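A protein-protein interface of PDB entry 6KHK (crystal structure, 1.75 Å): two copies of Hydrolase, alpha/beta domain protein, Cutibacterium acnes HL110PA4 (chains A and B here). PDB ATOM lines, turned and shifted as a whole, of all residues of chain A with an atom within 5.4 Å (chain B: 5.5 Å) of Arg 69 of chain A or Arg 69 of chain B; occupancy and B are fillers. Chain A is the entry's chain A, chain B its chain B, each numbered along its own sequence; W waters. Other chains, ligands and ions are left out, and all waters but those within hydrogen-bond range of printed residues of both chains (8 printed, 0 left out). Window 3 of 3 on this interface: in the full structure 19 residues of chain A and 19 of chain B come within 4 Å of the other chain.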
ATOM      1  N   GLU A   5     -15.990  12.237 -15.336  1.00  0.00           N
ATOM      2  CA  GLU A   5     -15.459  11.867 -16.656  1.00  0.00           C
ATOM      3  C   GLU A   5     -16.678  11.811 -17.562  1.00  0.00           C
ATOM      4  O   GLU A   5     -17.713  11.220 -17.210  1.00  0.00           O
ATOM      5  CB  GLU A   5     -14.643  10.581 -16.603  1.00  0.00           C
ATOM      6  CG  GLU A   5     -13.245  10.778 -16.055  1.00  0.00           C
ATOM      7  CD  GLU A   5     -12.412   9.510 -16.127  1.00  0.00           C
ATOM      8  OE1 GLU A   5     -12.894   8.556 -16.740  1.00  0.00           O
ATOM      9  OE2 GLU A   5     -11.306   9.456 -15.568  1.00  0.00           O
ATOM     10  N   GLN A  18     -13.001  12.914 -25.180  1.00  0.00           N
ATOM     11  CA  GLN A  18     -12.632  12.810 -23.741  1.00  0.00           C
ATOM     12  C   GLN A  18     -12.833  14.158 -23.049  1.00  0.00           C
ATOM     13  O   GLN A  18     -12.288  15.146 -23.517  1.00  0.00           O
ATOM     14  CB  GLN A  18     -11.177  12.364 -23.626  1.00  0.00           C
ATOM     15  CG  GLN A  18     -10.836  11.089 -24.406  1.00  0.00           C
ATOM     16  CD  GLN A  18     -11.595   9.913 -23.862  1.00  0.00           C
ATOM     17  OE1 GLN A  18     -11.350   9.488 -22.731  1.00  0.00           O
ATOM     18  NE2 GLN A  18     -12.527   9.402 -24.650  1.00  0.00           N
ATOM     19  N   TRP A  20     -13.892  16.320 -19.050  1.00  0.00           N
ATOM     20  CA  TRP A  20     -13.944  16.304 -17.575  1.00  0.00           C
ATOM     21  C   TRP A  20     -14.744  17.481 -17.065  1.00  0.00           C
ATOM     22  O   TRP A  20     -14.601  18.608 -17.635  1.00  0.00           O
ATOM     23  CB  TRP A  20     -12.526  16.357 -17.038  1.00  0.00           C
ATOM     24  CG  TRP A  20     -11.649  15.247 -17.523  1.00  0.00           C
ATOM     25  CD1 TRP A  20     -11.462  14.054 -16.894  1.00  0.00           C
ATOM     26  CD2 TRP A  20     -10.850  15.209 -18.714  1.00  0.00           C
ATOM     27  NE1 TRP A  20     -10.472  13.346 -17.508  1.00  0.00           N
ATOM     28  CE2 TRP A  20     -10.149  13.980 -18.684  1.00  0.00           C
ATOM     29  CE3 TRP A  20     -10.645  16.085 -19.791  1.00  0.00           C
ATOM     30  CZ2 TRP A  20      -9.254  13.622 -19.690  1.00  0.00           C
ATOM     31  CZ3 TRP A  20      -9.748  15.732 -20.778  1.00  0.00           C
ATOM     32  CH2 TRP A  20      -9.079  14.505 -20.742  1.00  0.00           C
ATOM     33  N   HIS A  41      -3.835  20.332 -25.041  1.00  0.00           N
ATOM     34  CA  HIS A  41      -4.895  19.522 -24.388  1.00  0.00           C
ATOM     35  C   HIS A  41      -5.436  20.228 -23.140  1.00  0.00           C
ATOM     36  O   HIS A  41      -4.815  21.187 -22.677  1.00  0.00           O
ATOM     37  CB  HIS A  41      -4.344  18.109 -24.151  1.00  0.00           C
ATOM     38  CG  HIS A  41      -3.298  18.094 -23.067  1.00  0.00           C
ATOM     39  ND1 HIS A  41      -3.582  17.698 -21.783  1.00  0.00           N
ATOM     40  CD2 HIS A  41      -1.981  18.401 -23.095  1.00  0.00           C
ATOM     41  CE1 HIS A  41      -2.470  17.698 -21.058  1.00  0.00           C
ATOM     42  NE2 HIS A  41      -1.474  18.173 -21.847  1.00  0.00           N
ATOM     43  N   ARG A  43      -5.888  19.201 -20.015  1.00  0.00           N
ATOM     44  CA  ARG A  43      -5.334  18.865 -18.678  1.00  0.00           C
ATOM     45  C   ARG A  43      -4.039  19.673 -18.454  1.00  0.00           C
ATOM     46  O   ARG A  43      -3.473  19.652 -17.358  1.00  0.00           O
ATOM     47  CB  ARG A  43      -5.310  17.326 -18.594  1.00  0.00           C
ATOM     48  CG  ARG A  43      -6.672  16.746 -18.271  1.00  0.00           C
ATOM     49  CD  ARG A  43      -6.679  15.251 -18.023  1.00  0.00           C
ATOM     50  NE  ARG A  43      -6.013  14.564 -19.082  1.00  0.00           N
ATOM     51  CZ  ARG A  43      -5.690  13.286 -19.083  1.00  0.00           C
ATOM     52  NH1 ARG A  43      -5.949  12.509 -18.043  1.00  0.00           N
ATOM     53  NH2 ARG A  43      -5.088  12.788 -20.126  1.00  0.00           N
ATOM     54  N   ASP A  63     -10.757  17.471 -24.525  1.00  0.00           N
ATOM     55  CA  ASP A  63      -9.674  17.383 -25.524  1.00  0.00           C
ATOM     56  C   ASP A  63     -10.384  17.299 -26.843  1.00  0.00           C
ATOM     57  O   ASP A  63     -11.191  16.336 -26.995  1.00  0.00           O
ATOM     58  CB  ASP A  63      -8.762  16.184 -25.265  1.00  0.00           C
ATOM     59  CG  ASP A  63      -7.978  16.361 -23.958  1.00  0.00           C
ATOM     60  OD1 ASP A  63      -8.014  17.461 -23.468  1.00  0.00           O
ATOM     61  OD2 ASP A  63      -7.223  15.470 -23.571  1.00  0.00           O
ATOM     62  N   HIS A  67      -6.841  15.729 -30.799  1.00  0.00           N
ATOM     63  CA  HIS A  67      -6.057  16.350 -29.704  1.00  0.00           C
ATOM     64  C   HIS A  67      -6.061  15.514 -28.420  1.00  0.00           C
ATOM     65  O   HIS A  67      -7.078  14.820 -28.108  1.00  0.00           O
ATOM     66  CB  HIS A  67      -6.620  17.758 -29.462  1.00  0.00           C
ATOM     67  CG  HIS A  67      -6.214  18.698 -30.548  1.00  0.00           C
ATOM     68  ND1 HIS A  67      -6.823  18.708 -31.784  1.00  0.00           N
ATOM     69  CD2 HIS A  67      -5.210  19.588 -30.587  1.00  0.00           C
ATOM     70  CE1 HIS A  67      -6.167  19.594 -32.538  1.00  0.00           C
ATOM     71  NE2 HIS A  67      -5.220  20.183 -31.799  1.00  0.00           N
ATOM     72  N   GLY A  68      -4.980  15.656 -27.676  1.00  0.00           N
ATOM     73  CA  GLY A  68      -4.838  15.136 -26.310  1.00  0.00           C
ATOM     74  C   GLY A  68      -5.294  13.708 -26.161  1.00  0.00           C
ATOM     75  O   GLY A  68      -4.896  12.829 -26.983  1.00  0.00           O
ATOM     76  N   ARG A  69      -6.110  13.435 -25.129  1.00  0.00           N
ATOM     77  CA  ARG A  69      -6.600  12.078 -24.795  1.00  0.00           C
ATOM     78  C   ARG A  69      -7.549  11.585 -25.874  1.00  0.00           C
ATOM     79  O   ARG A  69      -7.614  10.354 -26.092  1.00  0.00           O
ATOM     80  CB  ARG A  69      -7.260  12.015 -23.415  1.00  0.00           C
ATOM     81  CG  ARG A  69      -7.267  10.608 -22.845  1.00  0.00           C
ATOM     82  CD  ARG A  69      -7.820  10.523 -21.444  1.00  0.00           C
ATOM     83  NE  ARG A  69      -7.403   9.304 -20.787  1.00  0.00           N
ATOM     84  CZ  ARG A  69      -8.014   8.143 -20.936  1.00  0.00           C
ATOM     85  NH1 ARG A  69      -9.115   8.053 -21.646  1.00  0.00           N
ATOM     86  NH2 ARG A  69      -7.530   7.061 -20.368  1.00  0.00           N
ATOM     87  N   THR A  70      -8.292  12.482 -26.527  1.00  0.00           N
ATOM     88  CA  THR A  70      -9.157  12.108 -27.663  1.00  0.00           C
ATOM     89  C   THR A  70      -8.314  11.442 -28.767  1.00  0.00           C
ATOM     90  O   THR A  70      -8.669  10.338 -29.283  1.00  0.00           O
ATOM     91  CB  THR A  70      -9.957  13.348 -28.078  1.00  0.00           C
ATOM     92  OG1 THR A  70     -10.746  13.755 -26.947  1.00  0.00           O
ATOM     93  CG2 THR A  70     -10.802  13.025 -29.304  1.00  0.00           C
ATOM     94  N   ALA A  71      -7.220  12.062 -29.146  1.00  0.00           N
ATOM     95  CA  ALA A  71      -6.266  11.525 -30.130  1.00  0.00           C
ATOM     96  C   ALA A  71      -5.577  10.251 -29.612  1.00  0.00           C
ATOM     97  O   ALA A  71      -5.375   9.292 -30.390  1.00  0.00           O
ATOM     98  CB  ALA A  71      -5.277  12.609 -30.454  1.00  0.00           C
ATOM     99  N   MET A  72      -5.188  10.251 -28.363  1.00  0.00           N
ATOM    100  CA  MET A  72      -4.489   9.101 -27.750  1.00  0.00           C
ATOM    101  C   MET A  72      -5.437   7.883 -27.808  1.00  0.00           C
ATOM    102  O   MET A  72      -4.960   6.790 -28.177  1.00  0.00           O
ATOM    103  CB  MET A  72      -4.037   9.485 -26.330  1.00  0.00           C
ATOM    104  CG  MET A  72      -2.865   8.661 -25.767  1.00  0.00           C
ATOM    105  SD  MET A  72      -1.252   8.896 -26.492  1.00  0.00           S
ATOM    106  CE  MET A  72      -0.681  10.312 -25.548  1.00  0.00           C
ATOM    107  N   GLN A  73      -6.739   8.045 -27.537  1.00  0.00           N
ATOM    108  CA  GLN A  73      -7.729   6.934 -27.557  1.00  0.00           C
ATOM    109  C   GLN A  73      -8.121   6.544 -28.992  1.00  0.00           C
ATOM    110  O   GLN A  73      -8.327   5.365 -29.249  1.00  0.00           O
ATOM    111  CB  GLN A  73      -8.947   7.304 -26.712  1.00  0.00           C
ATOM    112  CG  GLN A  73      -8.630   7.412 -25.228  1.00  0.00           C
ATOM    113  CD  GLN A  73      -8.168   6.107 -24.617  1.00  0.00           C
ATOM    114  OE1 GLN A  73      -7.160   6.032 -23.922  1.00  0.00           O
ATOM    115  NE2 GLN A  73      -8.928   5.068 -24.857  1.00  0.00           N
ATOM    116  N   SER A  74      -8.248   7.487 -29.910  1.00  0.00           N
ATOM    117  CA  SER A  74      -8.692   7.224 -31.304  1.00  0.00           C
ATOM    118  C   SER A  74      -7.524   6.799 -32.217  1.00  0.00           C
ATOM    119  O   SER A  74      -7.804   6.172 -33.255  1.00  0.00           O
ATOM    120  CB  SER A  74      -9.379   8.446 -31.868  1.00  0.00           C
ATOM    121  OG  SER A  74      -8.397   9.432 -32.137  1.00  0.00           O
ATOM    122  N   PHE A 208       0.714  14.558 -24.280  1.00  0.00           N
ATOM    123  CA  PHE A 208      -0.685  14.860 -24.635  1.00  0.00           C
ATOM    124  C   PHE A 208      -0.825  16.111 -25.514  1.00  0.00           C
ATOM    125  O   PHE A 208      -1.973  16.410 -25.937  1.00  0.00           O
ATOM    126  CB  PHE A 208      -1.546  14.928 -23.380  1.00  0.00           C
ATOM    127  CG  PHE A 208      -1.791  13.569 -22.787  1.00  0.00           C
ATOM    128  CD1 PHE A 208      -0.960  13.087 -21.784  1.00  0.00           C
ATOM    129  CD2 PHE A 208      -2.826  12.757 -23.258  1.00  0.00           C
ATOM    130  CE1 PHE A 208      -1.146  11.816 -21.276  1.00  0.00           C
ATOM    131  CE2 PHE A 208      -3.026  11.490 -22.731  1.00  0.00           C
ATOM    132  CZ  PHE A 208      -2.158  11.016 -21.763  1.00  0.00           C
ATOM    133  N   GLU B   5       0.148   9.448 -18.332  1.00  0.00           N
ATOM    134  CA  GLU B   5      -0.806   8.409 -17.893  1.00  0.00           C
ATOM    135  C   GLU B   5      -0.009   7.124 -17.803  1.00  0.00           C
ATOM    136  O   GLU B   5       0.694   6.780 -18.777  1.00  0.00           O
ATOM    137  CB  GLU B   5      -1.976   8.229 -18.859  1.00  0.00           C
ATOM    138  CG  GLU B   5      -3.088   9.237 -18.603  1.00  0.00           C
ATOM    139  CD  GLU B   5      -4.265   9.106 -19.561  1.00  0.00           C
ATOM    140  OE1 GLU B   5      -4.378   8.075 -20.248  1.00  0.00           O
ATOM    141  OE2 GLU B   5      -5.106   9.985 -19.574  1.00  0.00           O
ATOM    142  N   GLN B  18      -4.810   2.566 -12.431  1.00  0.00           N
ATOM    143  CA  GLN B  18      -4.820   3.880 -13.105  1.00  0.00           C
ATOM    144  C   GLN B  18      -3.903   4.840 -12.332  1.00  0.00           C
ATOM    145  O   GLN B  18      -4.091   4.973 -11.155  1.00  0.00           O
ATOM    146  CB  GLN B  18      -6.269   4.389 -13.151  1.00  0.00           C
ATOM    147  CG  GLN B  18      -7.228   3.433 -13.834  1.00  0.00           C
ATOM    148  CD  GLN B  18      -6.859   3.128 -15.269  1.00  0.00           C
ATOM    149  OE1 GLN B  18      -6.945   4.010 -16.135  1.00  0.00           O
ATOM    150  NE2 GLN B  18      -6.471   1.880 -15.537  1.00  0.00           N
ATOM    151  N   TRP B  20      -1.081   8.546 -12.604  1.00  0.00           N
ATOM    152  CA  TRP B  20      -0.670   9.790 -13.303  1.00  0.00           C
ATOM    153  C   TRP B  20       0.669  10.275 -12.756  1.00  0.00           C
ATOM    154  O   TRP B  20       0.904  10.162 -11.520  1.00  0.00           O
ATOM    155  CB  TRP B  20      -1.730  10.893 -13.130  1.00  0.00           C
ATOM    156  CG  TRP B  20      -3.064  10.494 -13.672  1.00  0.00           C
ATOM    157  CD1 TRP B  20      -3.537  10.700 -14.935  1.00  0.00           C
ATOM    158  CD2 TRP B  20      -4.089   9.754 -12.979  1.00  0.00           C
ATOM    159  NE1 TRP B  20      -4.783  10.147 -15.069  1.00  0.00           N
ATOM    160  CE2 TRP B  20      -5.131   9.522 -13.906  1.00  0.00           C
ATOM    161  CE3 TRP B  20      -4.166   9.146 -11.730  1.00  0.00           C
ATOM    162  CZ2 TRP B  20      -6.276   8.814 -13.582  1.00  0.00           C
ATOM    163  CZ3 TRP B  20      -5.311   8.445 -11.404  1.00  0.00           C
ATOM    164  CH2 TRP B  20      -6.351   8.288 -12.317  1.00  0.00           C
ATOM    165  N   HIS B  41      -9.770   8.944  -3.895  1.00  0.00           N
ATOM    166  CA  HIS B  41      -9.012   8.792  -5.142  1.00  0.00           C
ATOM    167  C   HIS B  41      -7.971   9.902  -5.279  1.00  0.00           C
ATOM    168  O   HIS B  41      -8.081  10.886  -4.572  1.00  0.00           O
ATOM    169  CB  HIS B  41      -9.997   8.714  -6.340  1.00  0.00           C
ATOM    170  CG  HIS B  41     -10.707   9.989  -6.617  1.00  0.00           C
ATOM    171  ND1 HIS B  41     -10.300  10.872  -7.614  1.00  0.00           N
ATOM    172  CD2 HIS B  41     -11.831  10.508  -6.072  1.00  0.00           C
ATOM    173  CE1 HIS B  41     -11.113  11.903  -7.618  1.00  0.00           C
ATOM    174  NE2 HIS B  41     -12.062  11.716  -6.671  1.00  0.00           N
ATOM    175  N   ARG B  43      -7.137  11.934  -7.780  1.00  0.00           N
ATOM    176  CA  ARG B  43      -7.435  13.194  -8.504  1.00  0.00           C
ATOM    177  C   ARG B  43      -8.254  14.149  -7.605  1.00  0.00           C
ATOM    178  O   ARG B  43      -8.419  15.330  -7.942  1.00  0.00           O
ATOM    179  CB  ARG B  43      -8.071  12.834  -9.846  1.00  0.00           C
ATOM    180  CG  ARG B  43      -7.066  12.199 -10.817  1.00  0.00           C
ATOM    181  CD  ARG B  43      -7.725  12.011 -12.171  1.00  0.00           C
ATOM    182  NE  ARG B  43      -8.758  11.006 -12.139  1.00  0.00           N
ATOM    183  CZ  ARG B  43      -9.478  10.623 -13.206  1.00  0.00           C
ATOM    184  NH1 ARG B  43      -9.296  11.179 -14.395  1.00  0.00           N
ATOM    185  NH2 ARG B  43     -10.434   9.724 -13.063  1.00  0.00           N
ATOM    186  N   ASP B  63      -4.753   5.605  -8.285  1.00  0.00           N
ATOM    187  CA  ASP B  63      -5.996   5.152  -7.622  1.00  0.00           C
ATOM    188  C   ASP B  63      -5.774   3.701  -7.238  1.00  0.00           C
ATOM    189  O   ASP B  63      -5.686   2.831  -8.218  1.00  0.00           O
ATOM    190  CB  ASP B  63      -7.193   5.347  -8.566  1.00  0.00           C
ATOM    191  CG  ASP B  63      -7.557   6.811  -8.762  1.00  0.00           C
ATOM    192  OD1 ASP B  63      -6.924   7.651  -8.098  1.00  0.00           O
ATOM    193  OD2 ASP B  63      -8.471   7.104  -9.578  1.00  0.00           O
ATOM    194  N   HIS B  67     -10.504   1.265  -5.951  1.00  0.00           N
ATOM    195  CA  HIS B  67     -10.765   2.714  -5.710  1.00  0.00           C
ATOM    196  C   HIS B  67     -10.736   3.539  -6.989  1.00  0.00           C
ATOM    197  O   HIS B  67      -9.873   3.256  -7.870  1.00  0.00           O
ATOM    198  CB  HIS B  67      -9.714   3.304  -4.768  1.00  0.00           C
ATOM    199  CG  HIS B  67      -9.921   2.896  -3.355  1.00  0.00           C
ATOM    200  ND1 HIS B  67      -9.723   1.585  -2.916  1.00  0.00           N
ATOM    201  CD2 HIS B  67     -10.419   3.577  -2.310  1.00  0.00           C
ATOM    202  CE1 HIS B  67     -10.073   1.490  -1.661  1.00  0.00           C
ATOM    203  NE2 HIS B  67     -10.477   2.712  -1.225  1.00  0.00           N
ATOM    204  N   GLY B  68     -11.553   4.605  -7.027  1.00  0.00           N
ATOM    205  CA  GLY B  68     -11.288   5.690  -7.993  1.00  0.00           C
ATOM    206  C   GLY B  68     -11.439   5.149  -9.394  1.00  0.00           C
ATOM    207  O   GLY B  68     -12.287   4.294  -9.568  1.00  0.00           O
ATOM    208  N   ARG B  69     -10.578   5.562 -10.343  1.00  0.00           N
ATOM    209  CA  ARG B  69     -10.713   5.147 -11.773  1.00  0.00           C
ATOM    210  C   ARG B  69     -10.321   3.672 -11.918  1.00  0.00           C
ATOM    211  O   ARG B  69     -10.771   3.042 -12.825  1.00  0.00           O
ATOM    212  CB  ARG B  69      -9.815   6.001 -12.654  1.00  0.00           C
ATOM    213  CG  ARG B  69     -10.173   5.912 -14.128  1.00  0.00           C
ATOM    214  CD  ARG B  69      -9.297   6.874 -14.955  1.00  0.00           C
ATOM    215  NE  ARG B  69      -9.973   7.148 -16.226  1.00  0.00           N
ATOM    216  CZ  ARG B  69      -9.919   6.410 -17.325  1.00  0.00           C
ATOM    217  NH1 ARG B  69      -9.107   5.372 -17.418  1.00  0.00           N
ATOM    218  NH2 ARG B  69     -10.621   6.791 -18.383  1.00  0.00           N
ATOM    219  N   THR B  70      -9.454   3.154 -11.058  1.00  0.00           N
ATOM    220  CA  THR B  70      -9.130   1.707 -11.067  1.00  0.00           C
ATOM    221  C   THR B  70     -10.421   0.894 -10.865  1.00  0.00           C
ATOM    222  O   THR B  70     -10.620  -0.095 -11.608  1.00  0.00           O
ATOM    223  CB  THR B  70      -8.060   1.440  -9.999  1.00  0.00           C
ATOM    224  OG1 THR B  70      -6.906   2.221 -10.310  1.00  0.00           O
ATOM    225  CG2 THR B  70      -7.773  -0.038  -9.914  1.00  0.00           C
ATOM    226  N   ALA B  71     -11.254   1.286  -9.899  1.00  0.00           N
ATOM    227  CA  ALA B  71     -12.538   0.637  -9.588  1.00  0.00           C
ATOM    228  C   ALA B  71     -13.502   0.900 -10.752  1.00  0.00           C
ATOM    229  O   ALA B  71     -14.178  -0.061 -11.235  1.00  0.00           O
ATOM    230  CB  ALA B  71     -13.099   1.132  -8.276  1.00  0.00           C
ATOM    231  N   MET B  72     -13.556   2.150 -11.201  1.00  0.00           N
ATOM    232  CA  MET B  72     -14.452   2.533 -12.326  1.00  0.00           C
ATOM    233  C   MET B  72     -14.122   1.656 -13.552  1.00  0.00           C
ATOM    234  O   MET B  72     -15.081   1.113 -14.145  1.00  0.00           O
ATOM    235  CB  MET B  72     -14.361   4.047 -12.588  1.00  0.00           C
ATOM    236  CG  MET B  72     -15.537   4.618 -13.324  1.00  0.00           C
ATOM    237  SD  MET B  72     -17.083   4.737 -12.430  1.00  0.00           S
ATOM    238  CE  MET B  72     -16.769   6.207 -11.448  1.00  0.00           C
ATOM    239  N   GLN B  73     -12.845   1.360 -13.865  1.00  0.00           N
ATOM    240  CA  GLN B  73     -12.465   0.570 -15.071  1.00  0.00           C
ATOM    241  C   GLN B  73     -12.615  -0.949 -14.839  1.00  0.00           C
ATOM    242  O   GLN B  73     -13.004  -1.643 -15.796  1.00  0.00           O
ATOM    243  CB  GLN B  73     -11.056   0.916 -15.551  1.00  0.00           C
ATOM    244  CG  GLN B  73     -10.884   2.379 -15.951  1.00  0.00           C
ATOM    245  CD  GLN B  73     -11.652   2.734 -17.205  1.00  0.00           C
ATOM    246  OE1 GLN B  73     -12.467   3.669 -17.252  1.00  0.00           O
ATOM    247  NE2 GLN B  73     -11.427   1.925 -18.210  1.00  0.00           N
ATOM    248  N   SER B  74     -12.292  -1.460 -13.660  1.00  0.00           N
ATOM    249  CA  SER B  74     -12.438  -2.902 -13.313  1.00  0.00           C
ATOM    250  C   SER B  74     -13.886  -3.272 -12.940  1.00  0.00           C
ATOM    251  O   SER B  74     -14.234  -4.479 -13.026  1.00  0.00           O
ATOM    252  CB  SER B  74     -11.535  -3.238 -12.144  1.00  0.00           C
ATOM    253  OG  SER B  74     -12.074  -2.670 -10.968  1.00  0.00           O
ATOM    254  N   PHE B 208     -15.935   9.465  -8.090  1.00  0.00           N
ATOM    255  CA  PHE B 208     -14.673   8.699  -8.001  1.00  0.00           C
ATOM    256  C   PHE B 208     -14.324   8.343  -6.543  1.00  0.00           C
ATOM    257  O   PHE B 208     -13.383   7.539  -6.349  1.00  0.00           O
ATOM    258  CB  PHE B 208     -13.548   9.422  -8.759  1.00  0.00           C
ATOM    259  CG  PHE B 208     -13.757   9.288 -10.241  1.00  0.00           C
ATOM    260  CD1 PHE B 208     -14.590  10.183 -10.885  1.00  0.00           C
ATOM    261  CD2 PHE B 208     -13.183   8.247 -10.973  1.00  0.00           C
ATOM    262  CE1 PHE B 208     -14.837  10.059 -12.246  1.00  0.00           C
ATOM    263  CE2 PHE B 208     -13.435   8.117 -12.333  1.00  0.00           C
ATOM    264  CZ  PHE B 208     -14.259   9.029 -12.962  1.00  0.00           C
HETATM  265  O   HOH W   1      -7.245  13.160 -15.387  1.00  0.00           O
HETATM  266  O   HOH W   2      -8.610   4.240 -20.342  1.00  0.00           O
HETATM  267  O   HOH W   3     -10.756   5.363 -21.090  1.00  0.00           O
HETATM  268  O   HOH W   4     -11.008   9.968 -19.653  1.00  0.00           O
HETATM  269  O   HOH W   5      -6.758   9.491 -17.193  1.00  0.00           O
HETATM  270  O   HOH W   6      -9.389  10.625 -17.490  1.00  0.00           O
HETATM  271  O   HOH W   7      -4.799   8.025 -23.098  1.00  0.00           O
HETATM  272  O   HOH W   8     -13.456   5.877 -15.525  1.00  0.00           O
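The side-chain carboxylate (OE2) of Glu 5 of chain A is in salt-bridge range of the guanidinium group (NH2) of Arg 43 of chain B (2.7 Å).
The side-chain carboxylate (OE2) of Glu 5 of chain A is in salt-bridge range of the guanidinium group (NE) of Arg 69 of chain B.
The guanidinium group of Arg 43 of chain A is in salt-bridge range of the side-chain carboxylate of Glu 5 of chain B (2.9 Å).
The side-chain carboxylate (OE2) of Glu 5 of chain B lies within salt-bridge range of the guanidinium group (NE) of Arg 69 of chain A.
Among the printed residues, merely in contact across the chains: Glu 5 of chain A with Phe 208 of chain B (3.7 Å), Trp 20 of chain A with Arg 43 of chain B (3.97 Å), Arg 43 of chain A with Trp 20 of chain B (3.97 Å), Arg 69 of chain A with Arg 69 of chain B (3.7 Å) and Phe 208 of chain A with Glu 5 of chain B (3.6 Å).
Water W7 bridges OE1 of Glu 5 of chain B (2.9 Å) and OE1 of Gln 73 of chain A (3.2 Å).
Water W6 lies within hydrogen-bond range of the indole nitrogen of Trp 20 of chain A (2.9 Å), the side-chain carboxylate of Glu 5 of chain A (3.0 Å) and the guanidinium group of Arg 43 of chain B (3.1 Å).
Water W5 lies within hydrogen-bond range of OE2 of Glu 5 of chain B (2.9 Å), NE1 of Trp 20 of chain B (3.0 Å) and NH1 of Arg 43 of chain A (3.2 Å).
Water W1 bridges NH1 of Arg 43 of chain B and NH1 of Arg 43 of chain A.
Water W2 lies within hydrogen-bond range of the guanidinium group of Arg 69 of chain A (3.0 Å) and the guanidinium group of Arg 69 of chain B (3.2 Å).
Water W4 lies within hydrogen-bond range of the side-chain amide oxygen (OE1) of Gln 18 of chain A (3.1 Å), the guanidinium group (NH1) of Arg 69 of chain A (3.4 Å) and the guanidinium group (NH2) of Arg 69 of chain B (3.4 Å).
Arg 69 of chain A touches two residues of chain B.
Arg 69 of chain B touches just these residues of chain A: Glu 5 and Arg 69.
Of the printed residues of chain B, Trp 20 of chain A touches Arg 43.
Printed residues of chain B within 4 Å of Glu 5 of chain A: Arg 43, Arg 69 and Phe 208.
Of the printed residues of chain B, Arg 43 of chain A touches Glu 5 and Trp 20.
Gly 68 of chain B touches none of the printed residues of chain A.
The nearest residue of chain B that does not touch Arg 69 of chain A is Gln 18 of chain B (5.3 Å).
NH1 of Arg 69 of chain A sits at hydrogen-bond distance from OE1 of Gln 18 of chain A.
N of Arg 43 of chain A sits at hydrogen-bond distance from ND1 of His 41 of chain A.
The side-chain carboxylate (OD2) of Asp 63 of chain A sits at hydrogen-bond distance from the backbone NH (N) of Arg 69 of chain A.
The side-chain amide oxygen (OE1) of Gln 18 of chain B sits at hydrogen-bond distance from the guanidinium group (NH1) of Arg 69 of chain B, 2.9 Å away.
A ring nitrogen (ND1) of His 41 of chain B sits close to the backbone NH (N) of Arg 43 of chain B (3.3 Å).
The backbone NH (N) of Arg 69 of chain B lies within hydrogen-bond range of the side-chain carboxylate (OD2) of Asp 63 of chain B (2.7 Å).
Printed residues of chain B that touch a printed residue of chain A: Glu 5, Trp 20, Arg 43, Arg 69 and Phe 208.
Hydrophobic or aromatic side chains of chain B within 4 Å of the printed part of chain A: Trp 20 and Phe 208.
Along chain B the printed residues that touch a printed residue of chain A span positions 5 to 208.
Of the 15 printed residues of chain A, 5 touch a printed residue of chain B.
Hydrophobic or aromatic side chains of chain A that line the printed part of chain B: Trp 20 and Phe 208.
Among the printed residues, Asp or Glu carboxylates within 4 Å of a Lys or Arg side-chain nitrogen of the other chain: Glu 5 of chain A with Arg 43 of chain B, Glu 5 of chain A with Arg 69 of chain B, Arg 43 of chain A with Glu 5 of chain B and Arg 69 of chain A with Glu 5 of chain B.
Glu 5 of chain A touches Arg 69 of chain B, and with the chains exchanged Arg 69 of chain A touches Glu 5 of chain B.
Glu 5 of chain A touches Phe 208 of chain B, and with the chains exchanged Phe 208 of chain A touches Glu 5 of chain B.
Trp 20 of chain A touches Arg 43 of chain B, and with the chains exchanged Arg 43 of chain A touches Trp 20 of chain B.
Arg 69 of chain B touches its own counterpart, Arg 69 of chain A.
15 positions are printed for both chains.
Of the 9 pairs that touch across the chains among the printed residues, 9 have their exchanged pair printed and touching as well.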
